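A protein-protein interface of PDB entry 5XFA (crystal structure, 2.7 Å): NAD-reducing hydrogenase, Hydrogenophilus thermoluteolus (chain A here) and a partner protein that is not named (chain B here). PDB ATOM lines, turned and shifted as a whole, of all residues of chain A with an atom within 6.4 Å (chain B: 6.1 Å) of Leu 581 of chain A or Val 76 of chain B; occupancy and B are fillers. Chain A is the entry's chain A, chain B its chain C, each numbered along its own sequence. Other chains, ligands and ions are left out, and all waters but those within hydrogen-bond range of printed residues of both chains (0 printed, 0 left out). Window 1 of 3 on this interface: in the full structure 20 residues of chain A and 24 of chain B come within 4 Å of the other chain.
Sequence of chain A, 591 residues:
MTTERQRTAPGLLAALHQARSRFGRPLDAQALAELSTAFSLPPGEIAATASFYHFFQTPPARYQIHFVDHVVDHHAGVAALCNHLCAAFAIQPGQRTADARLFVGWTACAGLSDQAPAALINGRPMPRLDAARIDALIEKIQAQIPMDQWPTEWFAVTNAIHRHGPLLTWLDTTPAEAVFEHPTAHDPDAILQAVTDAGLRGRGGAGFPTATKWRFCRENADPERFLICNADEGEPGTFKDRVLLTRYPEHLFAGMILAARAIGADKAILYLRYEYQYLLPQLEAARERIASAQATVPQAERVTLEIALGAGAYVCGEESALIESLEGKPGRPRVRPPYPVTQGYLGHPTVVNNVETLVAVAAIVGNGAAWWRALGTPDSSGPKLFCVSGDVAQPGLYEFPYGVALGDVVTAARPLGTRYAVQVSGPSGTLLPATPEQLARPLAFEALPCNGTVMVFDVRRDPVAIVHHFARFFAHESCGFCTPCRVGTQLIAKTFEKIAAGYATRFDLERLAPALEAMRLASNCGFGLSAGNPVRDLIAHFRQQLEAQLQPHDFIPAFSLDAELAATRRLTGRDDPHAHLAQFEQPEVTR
Printed residues of chain B that touch a printed residue of chain A: Val 76, Glu 77, Arg 80 and Leu 140. Hydrophobic or aromatic side chains of chain B within 4 Å of the printed part of chain A: Val 76 and Leu 140. Of the 11 printed residues of chain A, 5 touch a printed residue of chain B. Printed residues of chain A that touch a printed residue of chain B: Leu 561, Leu 565, Leu 581, Ala 582 and Gln 583. Hydrophobic or aromatic side chains of chain A within 4 Å of the printed part of chain B: Leu 561, Leu 565 and Leu 581. Along chain A the printed residues that touch a printed residue of chain B span positions 561 to 583. Among the printed residues, no Asp or Glu carboxylate lies within 4 Å of a Lys or Arg side-chain nitrogen of the other chain.
The side-chain amide oxygen (OE1) of Gln 583 of chain A sits at hydrogen-bond distance from the backbone NH (N) of Leu 561 of chain A.
Leu 581 of chain A touches just these residues of chain B: Val 76 (3.9 Å) and Glu 77 (3.2 Å). Val 76 of chain B touches just one residue of chain A: Leu 581 (3.9 Å). Of the printed residues of chain B, Ala 582 of chain A touches Arg 80. Of the printed residues of chain B, Gln 583 of chain A touches Arg 80 (3.6 Å). Printed residues of chain A within 4 Å of Arg 80 of chain B: Leu 561 (3.3 Å), Ala 582 (2.5 Å) and Gln 583 (3.6 Å). Printed residues of chain A within 4 Å of Leu 140 of chain B: Leu 565 (3.6 Å). The nearest printed residue of chain B that does not touch Ala 582 of chain A is Val 76 of chain B (5.6 Å).
NH1 of Arg 80 of chain B sits at hydrogen-bond distance from O of Ala 582 of chain A, at 2.5 Å.
Among the printed residues, merely in contact across the chains: Leu 561 of chain A with Arg 80 of chain B, Leu 565 of chain A with Leu 140 of chain B, Leu 581 of chain A with Val 76 of chain B, Leu 581 of chain A with Glu 77 of chain B and Gln 583 of chain A with Arg 80 of chain B.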
ATOM      1  N   LEU A 561      -1.942  24.126  -2.912  1.00  0.00           N
ATOM      2  CA  LEU A 561      -0.973  24.279  -3.990  1.00  0.00           C
ATOM      3  C   LEU A 561      -0.200  25.607  -3.982  1.00  0.00           C
ATOM      4  O   LEU A 561       0.617  25.841  -4.878  1.00  0.00           O
ATOM      5  CB  LEU A 561      -1.733  24.108  -5.283  1.00  0.00           C
ATOM      6  CG  LEU A 561      -1.997  22.646  -5.661  1.00  0.00           C
ATOM      7  CD1 LEU A 561      -3.033  22.562  -6.761  1.00  0.00           C
ATOM      8  CD2 LEU A 561      -0.729  21.964  -6.115  1.00  0.00           C
ATOM      9  N   ASP A 562      -0.426  26.447  -2.961  1.00  0.00           N
ATOM     10  CA  ASP A 562       0.406  27.622  -2.713  1.00  0.00           C
ATOM     11  C   ASP A 562      -0.065  28.393  -1.498  1.00  0.00           C
ATOM     12  O   ASP A 562      -1.085  29.079  -1.609  1.00  0.00           O
ATOM     13  CB  ASP A 562       0.358  28.571  -3.921  1.00  0.00           C
ATOM     14  CG  ASP A 562      -1.069  28.912  -4.361  1.00  0.00           C
ATOM     15  OD1 ASP A 562      -1.956  28.044  -4.184  1.00  0.00           O
ATOM     16  OD2 ASP A 562      -1.293  30.039  -4.889  1.00  0.00           O
ATOM     17  N   LEU A 565       4.060  26.988  -3.514  1.00  0.00           N
ATOM     18  CA  LEU A 565       4.848  28.016  -4.213  1.00  0.00           C
ATOM     19  C   LEU A 565       5.268  29.228  -3.332  1.00  0.00           C
ATOM     20  O   LEU A 565       5.980  30.127  -3.800  1.00  0.00           O
ATOM     21  CB  LEU A 565       4.080  28.501  -5.439  1.00  0.00           C
ATOM     22  CG  LEU A 565       3.709  27.389  -6.409  1.00  0.00           C
ATOM     23  CD1 LEU A 565       2.655  27.850  -7.398  1.00  0.00           C
ATOM     24  CD2 LEU A 565       4.939  26.901  -7.142  1.00  0.00           C
ATOM     25  N   ARG A 569       8.089  31.825  -4.424  1.00  0.00           N
ATOM     26  CA  ARG A 569       7.659  33.237  -4.528  1.00  0.00           C
ATOM     27  C   ARG A 569       8.533  34.174  -3.662  1.00  0.00           C
ATOM     28  O   ARG A 569       9.109  35.123  -4.173  1.00  0.00           O
ATOM     29  CB  ARG A 569       6.176  33.412  -4.195  1.00  0.00           C
ATOM     30  CG  ARG A 569       5.260  33.203  -5.399  1.00  0.00           C
ATOM     31  CD  ARG A 569       3.875  33.747  -5.138  1.00  0.00           C
ATOM     32  NE  ARG A 569       3.294  33.129  -3.948  1.00  0.00           N
ATOM     33  CZ  ARG A 569       2.521  32.049  -3.949  1.00  0.00           C
ATOM     34  NH1 ARG A 569       2.199  31.443  -5.094  1.00  0.00           N
ATOM     35  NH2 ARG A 569       2.060  31.578  -2.796  1.00  0.00           N
ATOM     36  N   PRO A 577       0.365  36.199 -11.949  1.00  0.00           N
ATOM     37  CA  PRO A 577      -0.508  35.016 -12.011  1.00  0.00           C
ATOM     38  C   PRO A 577       0.229  33.679 -12.197  1.00  0.00           C
ATOM     39  O   PRO A 577      -0.037  32.711 -11.487  1.00  0.00           O
ATOM     40  CB  PRO A 577      -1.384  35.301 -13.236  1.00  0.00           C
ATOM     41  CG  PRO A 577      -0.716  36.432 -13.972  1.00  0.00           C
ATOM     42  CD  PRO A 577      -0.087  37.241 -12.886  1.00  0.00           C
ATOM     43  N   HIS A 578       1.169  33.640 -13.135  1.00  0.00           N
ATOM     44  CA  HIS A 578       1.966  32.426 -13.407  1.00  0.00           C
ATOM     45  C   HIS A 578       2.800  31.906 -12.231  1.00  0.00           C
ATOM     46  O   HIS A 578       3.332  30.825 -12.325  1.00  0.00           O
ATOM     47  CB  HIS A 578       2.879  32.656 -14.619  1.00  0.00           C
ATOM     48  CG  HIS A 578       2.134  32.693 -15.922  1.00  0.00           C
ATOM     49  ND1 HIS A 578       1.844  31.558 -16.654  1.00  0.00           N
ATOM     50  CD2 HIS A 578       1.589  33.727 -16.606  1.00  0.00           C
ATOM     51  CE1 HIS A 578       1.181  31.893 -17.745  1.00  0.00           C
ATOM     52  NE2 HIS A 578       1.007  33.203 -17.736  1.00  0.00           N
ATOM     53  N   ALA A 579       2.933  32.674 -11.149  1.00  0.00           N
ATOM     54  CA  ALA A 579       3.567  32.200  -9.898  1.00  0.00           C
ATOM     55  C   ALA A 579       2.544  31.784  -8.830  1.00  0.00           C
ATOM     56  O   ALA A 579       2.858  31.770  -7.622  1.00  0.00           O
ATOM     57  CB  ALA A 579       4.480  33.273  -9.328  1.00  0.00           C
ATOM     58  N   HIS A 580       1.334  31.458  -9.301  1.00  0.00           N
ATOM     59  CA  HIS A 580       0.218  31.033  -8.466  1.00  0.00           C
ATOM     60  C   HIS A 580      -0.503  29.876  -9.143  1.00  0.00           C
ATOM     61  O   HIS A 580      -0.632  29.851 -10.372  1.00  0.00           O
ATOM     62  CB  HIS A 580      -0.769  32.185  -8.266  1.00  0.00           C
ATOM     63  CG  HIS A 580      -0.281  33.239  -7.329  1.00  0.00           C
ATOM     64  ND1 HIS A 580      -0.318  33.090  -5.958  1.00  0.00           N
ATOM     65  CD2 HIS A 580       0.255  34.455  -7.559  1.00  0.00           C
ATOM     66  CE1 HIS A 580       0.183  34.169  -5.384  1.00  0.00           C
ATOM     67  NE2 HIS A 580       0.535  35.014  -6.336  1.00  0.00           N
ATOM     68  N   LEU A 581      -0.984  28.927  -8.344  1.00  0.00           N
ATOM     69  CA  LEU A 581      -1.763  27.809  -8.869  1.00  0.00           C
ATOM     70  C   LEU A 581      -3.133  27.797  -8.263  1.00  0.00           C
ATOM     71  O   LEU A 581      -3.291  28.125  -7.098  1.00  0.00           O
ATOM     72  CB  LEU A 581      -1.085  26.473  -8.569  1.00  0.00           C
ATOM     73  CG  LEU A 581       0.028  26.088  -9.532  1.00  0.00           C
ATOM     74  CD1 LEU A 581       0.761  24.877  -8.985  1.00  0.00           C
ATOM     75  CD2 LEU A 581      -0.509  25.840 -10.941  1.00  0.00           C
ATOM     76  N   ALA A 582      -4.109  27.391  -9.067  1.00  0.00           N
ATOM     77  CA  ALA A 582      -5.458  27.163  -8.591  1.00  0.00           C
ATOM     78  C   ALA A 582      -5.528  25.752  -8.088  1.00  0.00           C
ATOM     79  O   ALA A 582      -4.829  24.880  -8.595  1.00  0.00           O
ATOM     80  CB  ALA A 582      -6.467  27.346  -9.718  1.00  0.00           C
ATOM     81  N   GLN A 583      -6.367  25.527  -7.085  1.00  0.00           N
ATOM     82  CA  GLN A 583      -6.852  24.183  -6.819  1.00  0.00           C
ATOM     83  C   GLN A 583      -8.098  23.973  -7.654  1.00  0.00           C
ATOM     84  O   GLN A 583      -8.491  24.852  -8.441  1.00  0.00           O
ATOM     85  CB  GLN A 583      -7.121  23.982  -5.341  1.00  0.00           C
ATOM     86  CG  GLN A 583      -6.593  22.655  -4.860  1.00  0.00           C
ATOM     87  CD  GLN A 583      -5.751  22.856  -3.656  1.00  0.00           C
ATOM     88  OE1 GLN A 583      -4.933  23.761  -3.640  1.00  0.00           O
ATOM     89  NE2 GLN A 583      -5.928  22.025  -2.650  1.00  0.00           N
ATOM     90  N   LEU B  21       6.805  14.975 -17.019  1.00  0.00           N
ATOM     91  CA  LEU B  21       6.754  16.037 -16.016  1.00  0.00           C
ATOM     92  C   LEU B  21       8.154  16.145 -15.397  1.00  0.00           C
ATOM     93  O   LEU B  21       9.094  16.406 -16.120  1.00  0.00           O
ATOM     94  CB  LEU B  21       5.647  15.747 -15.025  1.00  0.00           C
ATOM     95  CG  LEU B  21       4.318  15.479 -15.720  1.00  0.00           C
ATOM     96  CD1 LEU B  21       3.276  14.968 -14.751  1.00  0.00           C
ATOM     97  CD2 LEU B  21       3.838  16.723 -16.421  1.00  0.00           C
ATOM     98  N   VAL B  70       5.643  15.588 -10.074  1.00  0.00           N
ATOM     99  CA  VAL B  70       5.330  17.020 -10.257  1.00  0.00           C
ATOM    100  C   VAL B  70       6.253  17.787  -9.342  1.00  0.00           C
ATOM    101  O   VAL B  70       6.301  17.537  -8.127  1.00  0.00           O
ATOM    102  CB  VAL B  70       3.846  17.403 -10.051  1.00  0.00           C
ATOM    103  CG1 VAL B  70       2.972  16.552 -10.952  1.00  0.00           C
ATOM    104  CG2 VAL B  70       3.412  17.251  -8.608  1.00  0.00           C
ATOM    105  N   ASN B  72       7.201  21.400 -10.351  1.00  0.00           N
ATOM    106  CA  ASN B  72       7.035  22.819 -10.560  1.00  0.00           C
ATOM    107  C   ASN B  72       5.640  23.126 -11.092  1.00  0.00           C
ATOM    108  O   ASN B  72       4.866  22.224 -11.413  1.00  0.00           O
ATOM    109  CB  ASN B  72       8.120  23.345 -11.501  1.00  0.00           C
ATOM    110  CG  ASN B  72       7.964  22.845 -12.918  1.00  0.00           C
ATOM    111  OD1 ASN B  72       6.933  23.066 -13.562  1.00  0.00           O
ATOM    112  ND2 ASN B  72       9.009  22.202 -13.436  1.00  0.00           N
ATOM    113  N   ALA B  73       5.336  24.411 -11.188  1.00  0.00           N
ATOM    114  CA  ALA B  73       3.996  24.863 -11.517  1.00  0.00           C
ATOM    115  C   ALA B  73       3.537  24.400 -12.898  1.00  0.00           C
ATOM    116  O   ALA B  73       2.407  23.958 -13.041  1.00  0.00           O
ATOM    117  CB  ALA B  73       3.911  26.381 -11.401  1.00  0.00           C
ATOM    118  N   GLU B  74       4.402  24.469 -13.902  1.00  0.00           N
ATOM    119  CA  GLU B  74       3.988  24.065 -15.239  1.00  0.00           C
ATOM    120  C   GLU B  74       3.706  22.544 -15.332  1.00  0.00           C
ATOM    121  O   GLU B  74       2.926  22.106 -16.183  1.00  0.00           O
ATOM    122  CB  GLU B  74       4.981  24.537 -16.324  1.00  0.00           C
ATOM    123  CG  GLU B  74       4.325  24.614 -17.705  1.00  0.00           C
ATOM    124  CD  GLU B  74       5.259  24.402 -18.886  1.00  0.00           C
ATOM    125  OE1 GLU B  74       6.246  23.642 -18.767  1.00  0.00           O
ATOM    126  OE2 GLU B  74       4.970  24.972 -19.963  1.00  0.00           O
ATOM    127  N   ASN B  75       4.300  21.741 -14.451  1.00  0.00           N
ATOM    128  CA  ASN B  75       3.957  20.319 -14.409  1.00  0.00           C
ATOM    129  C   ASN B  75       2.501  20.147 -14.028  1.00  0.00           C
ATOM    130  O   ASN B  75       1.820  19.275 -14.556  1.00  0.00           O
ATOM    131  CB  ASN B  75       4.781  19.541 -13.390  1.00  0.00           C
ATOM    132  CG  ASN B  75       6.232  19.431 -13.743  1.00  0.00           C
ATOM    133  OD1 ASN B  75       7.070  19.209 -12.853  1.00  0.00           O
ATOM    134  ND2 ASN B  75       6.555  19.582 -15.033  1.00  0.00           N
ATOM    135  N   VAL B  76       2.033  20.972 -13.095  1.00  0.00           N
ATOM    136  CA  VAL B  76       0.674  20.842 -12.608  1.00  0.00           C
ATOM    137  C   VAL B  76      -0.301  21.223 -13.710  1.00  0.00           C
ATOM    138  O   VAL B  76      -1.234  20.483 -13.996  1.00  0.00           O
ATOM    139  CB  VAL B  76       0.445  21.663 -11.324  1.00  0.00           C
ATOM    140  CG1 VAL B  76      -0.992  21.525 -10.842  1.00  0.00           C
ATOM    141  CG2 VAL B  76       1.400  21.208 -10.225  1.00  0.00           C
ATOM    142  N   GLU B  77      -0.075  22.365 -14.346  1.00  0.00           N
ATOM    143  CA  GLU B  77      -0.969  22.843 -15.423  1.00  0.00           C
ATOM    144  C   GLU B  77      -1.075  21.827 -16.535  1.00  0.00           C
ATOM    145  O   GLU B  77      -2.159  21.542 -16.998  1.00  0.00           O
ATOM    146  CB  GLU B  77      -0.525  24.218 -15.955  1.00  0.00           C
ATOM    147  CG  GLU B  77      -1.035  25.390 -15.086  1.00  0.00           C
ATOM    148  CD  GLU B  77      -0.042  26.554 -14.934  1.00  0.00           C
ATOM    149  OE1 GLU B  77       0.031  27.134 -13.828  1.00  0.00           O
ATOM    150  OE2 GLU B  77       0.658  26.900 -15.915  1.00  0.00           O
ATOM    151  N   VAL B  78       0.056  21.244 -16.900  1.00  0.00           N
ATOM    152  CA  VAL B  78       0.117  20.214 -17.940  1.00  0.00           C
ATOM    153  C   VAL B  78      -0.557  18.901 -17.524  1.00  0.00           C
ATOM    154  O   VAL B  78      -1.330  18.332 -18.285  1.00  0.00           O
ATOM    155  CB  VAL B  78       1.581  19.909 -18.333  1.00  0.00           C
ATOM    156  CG1 VAL B  78       1.661  18.673 -19.212  1.00  0.00           C
ATOM    157  CG2 VAL B  78       2.196  21.104 -19.049  1.00  0.00           C
ATOM    158  N   LEU B  79      -0.266  18.433 -16.312  1.00  0.00           N
ATOM    159  CA  LEU B  79      -0.862  17.201 -15.785  1.00  0.00           C
ATOM    160  C   LEU B  79      -2.383  17.266 -15.781  1.00  0.00           C
ATOM    161  O   LEU B  79      -3.051  16.324 -16.214  1.00  0.00           O
ATOM    162  CB  LEU B  79      -0.367  16.931 -14.369  1.00  0.00           C
ATOM    163  CG  LEU B  79      -0.937  15.682 -13.682  1.00  0.00           C
ATOM    164  CD1 LEU B  79      -0.693  14.447 -14.540  1.00  0.00           C
ATOM    165  CD2 LEU B  79      -0.339  15.508 -12.296  1.00  0.00           C
ATOM    166  N   ARG B  80      -2.914  18.389 -15.297  1.00  0.00           N
ATOM    167  CA  ARG B  80      -4.347  18.650 -15.293  1.00  0.00           C
ATOM    168  C   ARG B  80      -4.881  18.639 -16.699  1.00  0.00           C
ATOM    169  O   ARG B  80      -5.955  18.083 -16.935  1.00  0.00           O
ATOM    170  CB  ARG B  80      -4.642  19.997 -14.649  1.00  0.00           C
ATOM    171  CG  ARG B  80      -4.452  19.947 -13.151  1.00  0.00           C
ATOM    172  CD  ARG B  80      -4.637  21.283 -12.441  1.00  0.00           C
ATOM    173  NE  ARG B  80      -5.085  21.048 -11.069  1.00  0.00           N
ATOM    174  CZ  ARG B  80      -4.962  21.906 -10.067  1.00  0.00           C
ATOM    175  NH1 ARG B  80      -4.389  23.093 -10.251  1.00  0.00           N
ATOM    176  NH2 ARG B  80      -5.420  21.565  -8.862  1.00  0.00           N
ATOM    177  N   ALA B  81      -4.155  19.258 -17.635  1.00  0.00           N
ATOM    178  CA  ALA B  81      -4.615  19.304 -19.005  1.00  0.00           C
ATOM    179  C   ALA B  81      -4.773  17.894 -19.532  1.00  0.00           C
ATOM    180  O   ALA B  81      -5.836  17.518 -20.030  1.00  0.00           O
ATOM    181  CB  ALA B  81      -3.643  20.080 -19.877  1.00  0.00           C
ATOM    182  N   LEU B 140       7.779  23.722  -6.655  1.00  0.00           N
ATOM    183  CA  LEU B 140       6.931  23.472  -5.486  1.00  0.00           C
ATOM    184  C   LEU B 140       7.795  23.187  -4.277  1.00  0.00           C
ATOM    185  O   LEU B 140       8.980  22.903  -4.396  1.00  0.00           O
ATOM    186  CB  LEU B 140       5.984  22.289  -5.730  1.00  0.00           C
ATOM    187  CG  LEU B 140       4.733  22.511  -6.599  1.00  0.00           C
ATOM    188  CD1 LEU B 140       5.032  23.377  -7.799  1.00  0.00           C
ATOM    189  CD2 LEU B 140       4.184  21.185  -7.094  1.00  0.00           C
ATOM    190  N   ILE B 149      -2.114  14.841  -7.190  1.00  0.00           N
ATOM    191  CA  ILE B 149      -2.653  15.966  -7.949  1.00  0.00           C
ATOM    192  C   ILE B 149      -3.878  15.576  -8.765  1.00  0.00           C
ATOM    193  O   ILE B 149      -4.852  16.317  -8.797  1.00  0.00           O
ATOM    194  CB  ILE B 149      -1.573  16.524  -8.895  1.00  0.00           C
ATOM    195  CG1 ILE B 149      -0.324  16.958  -8.103  1.00  0.00           C
ATOM    196  CG2 ILE B 149      -2.107  17.674  -9.740  1.00  0.00           C
ATOM    197  CD1 ILE B 149      -0.558  18.019  -7.041  1.00  0.00           C
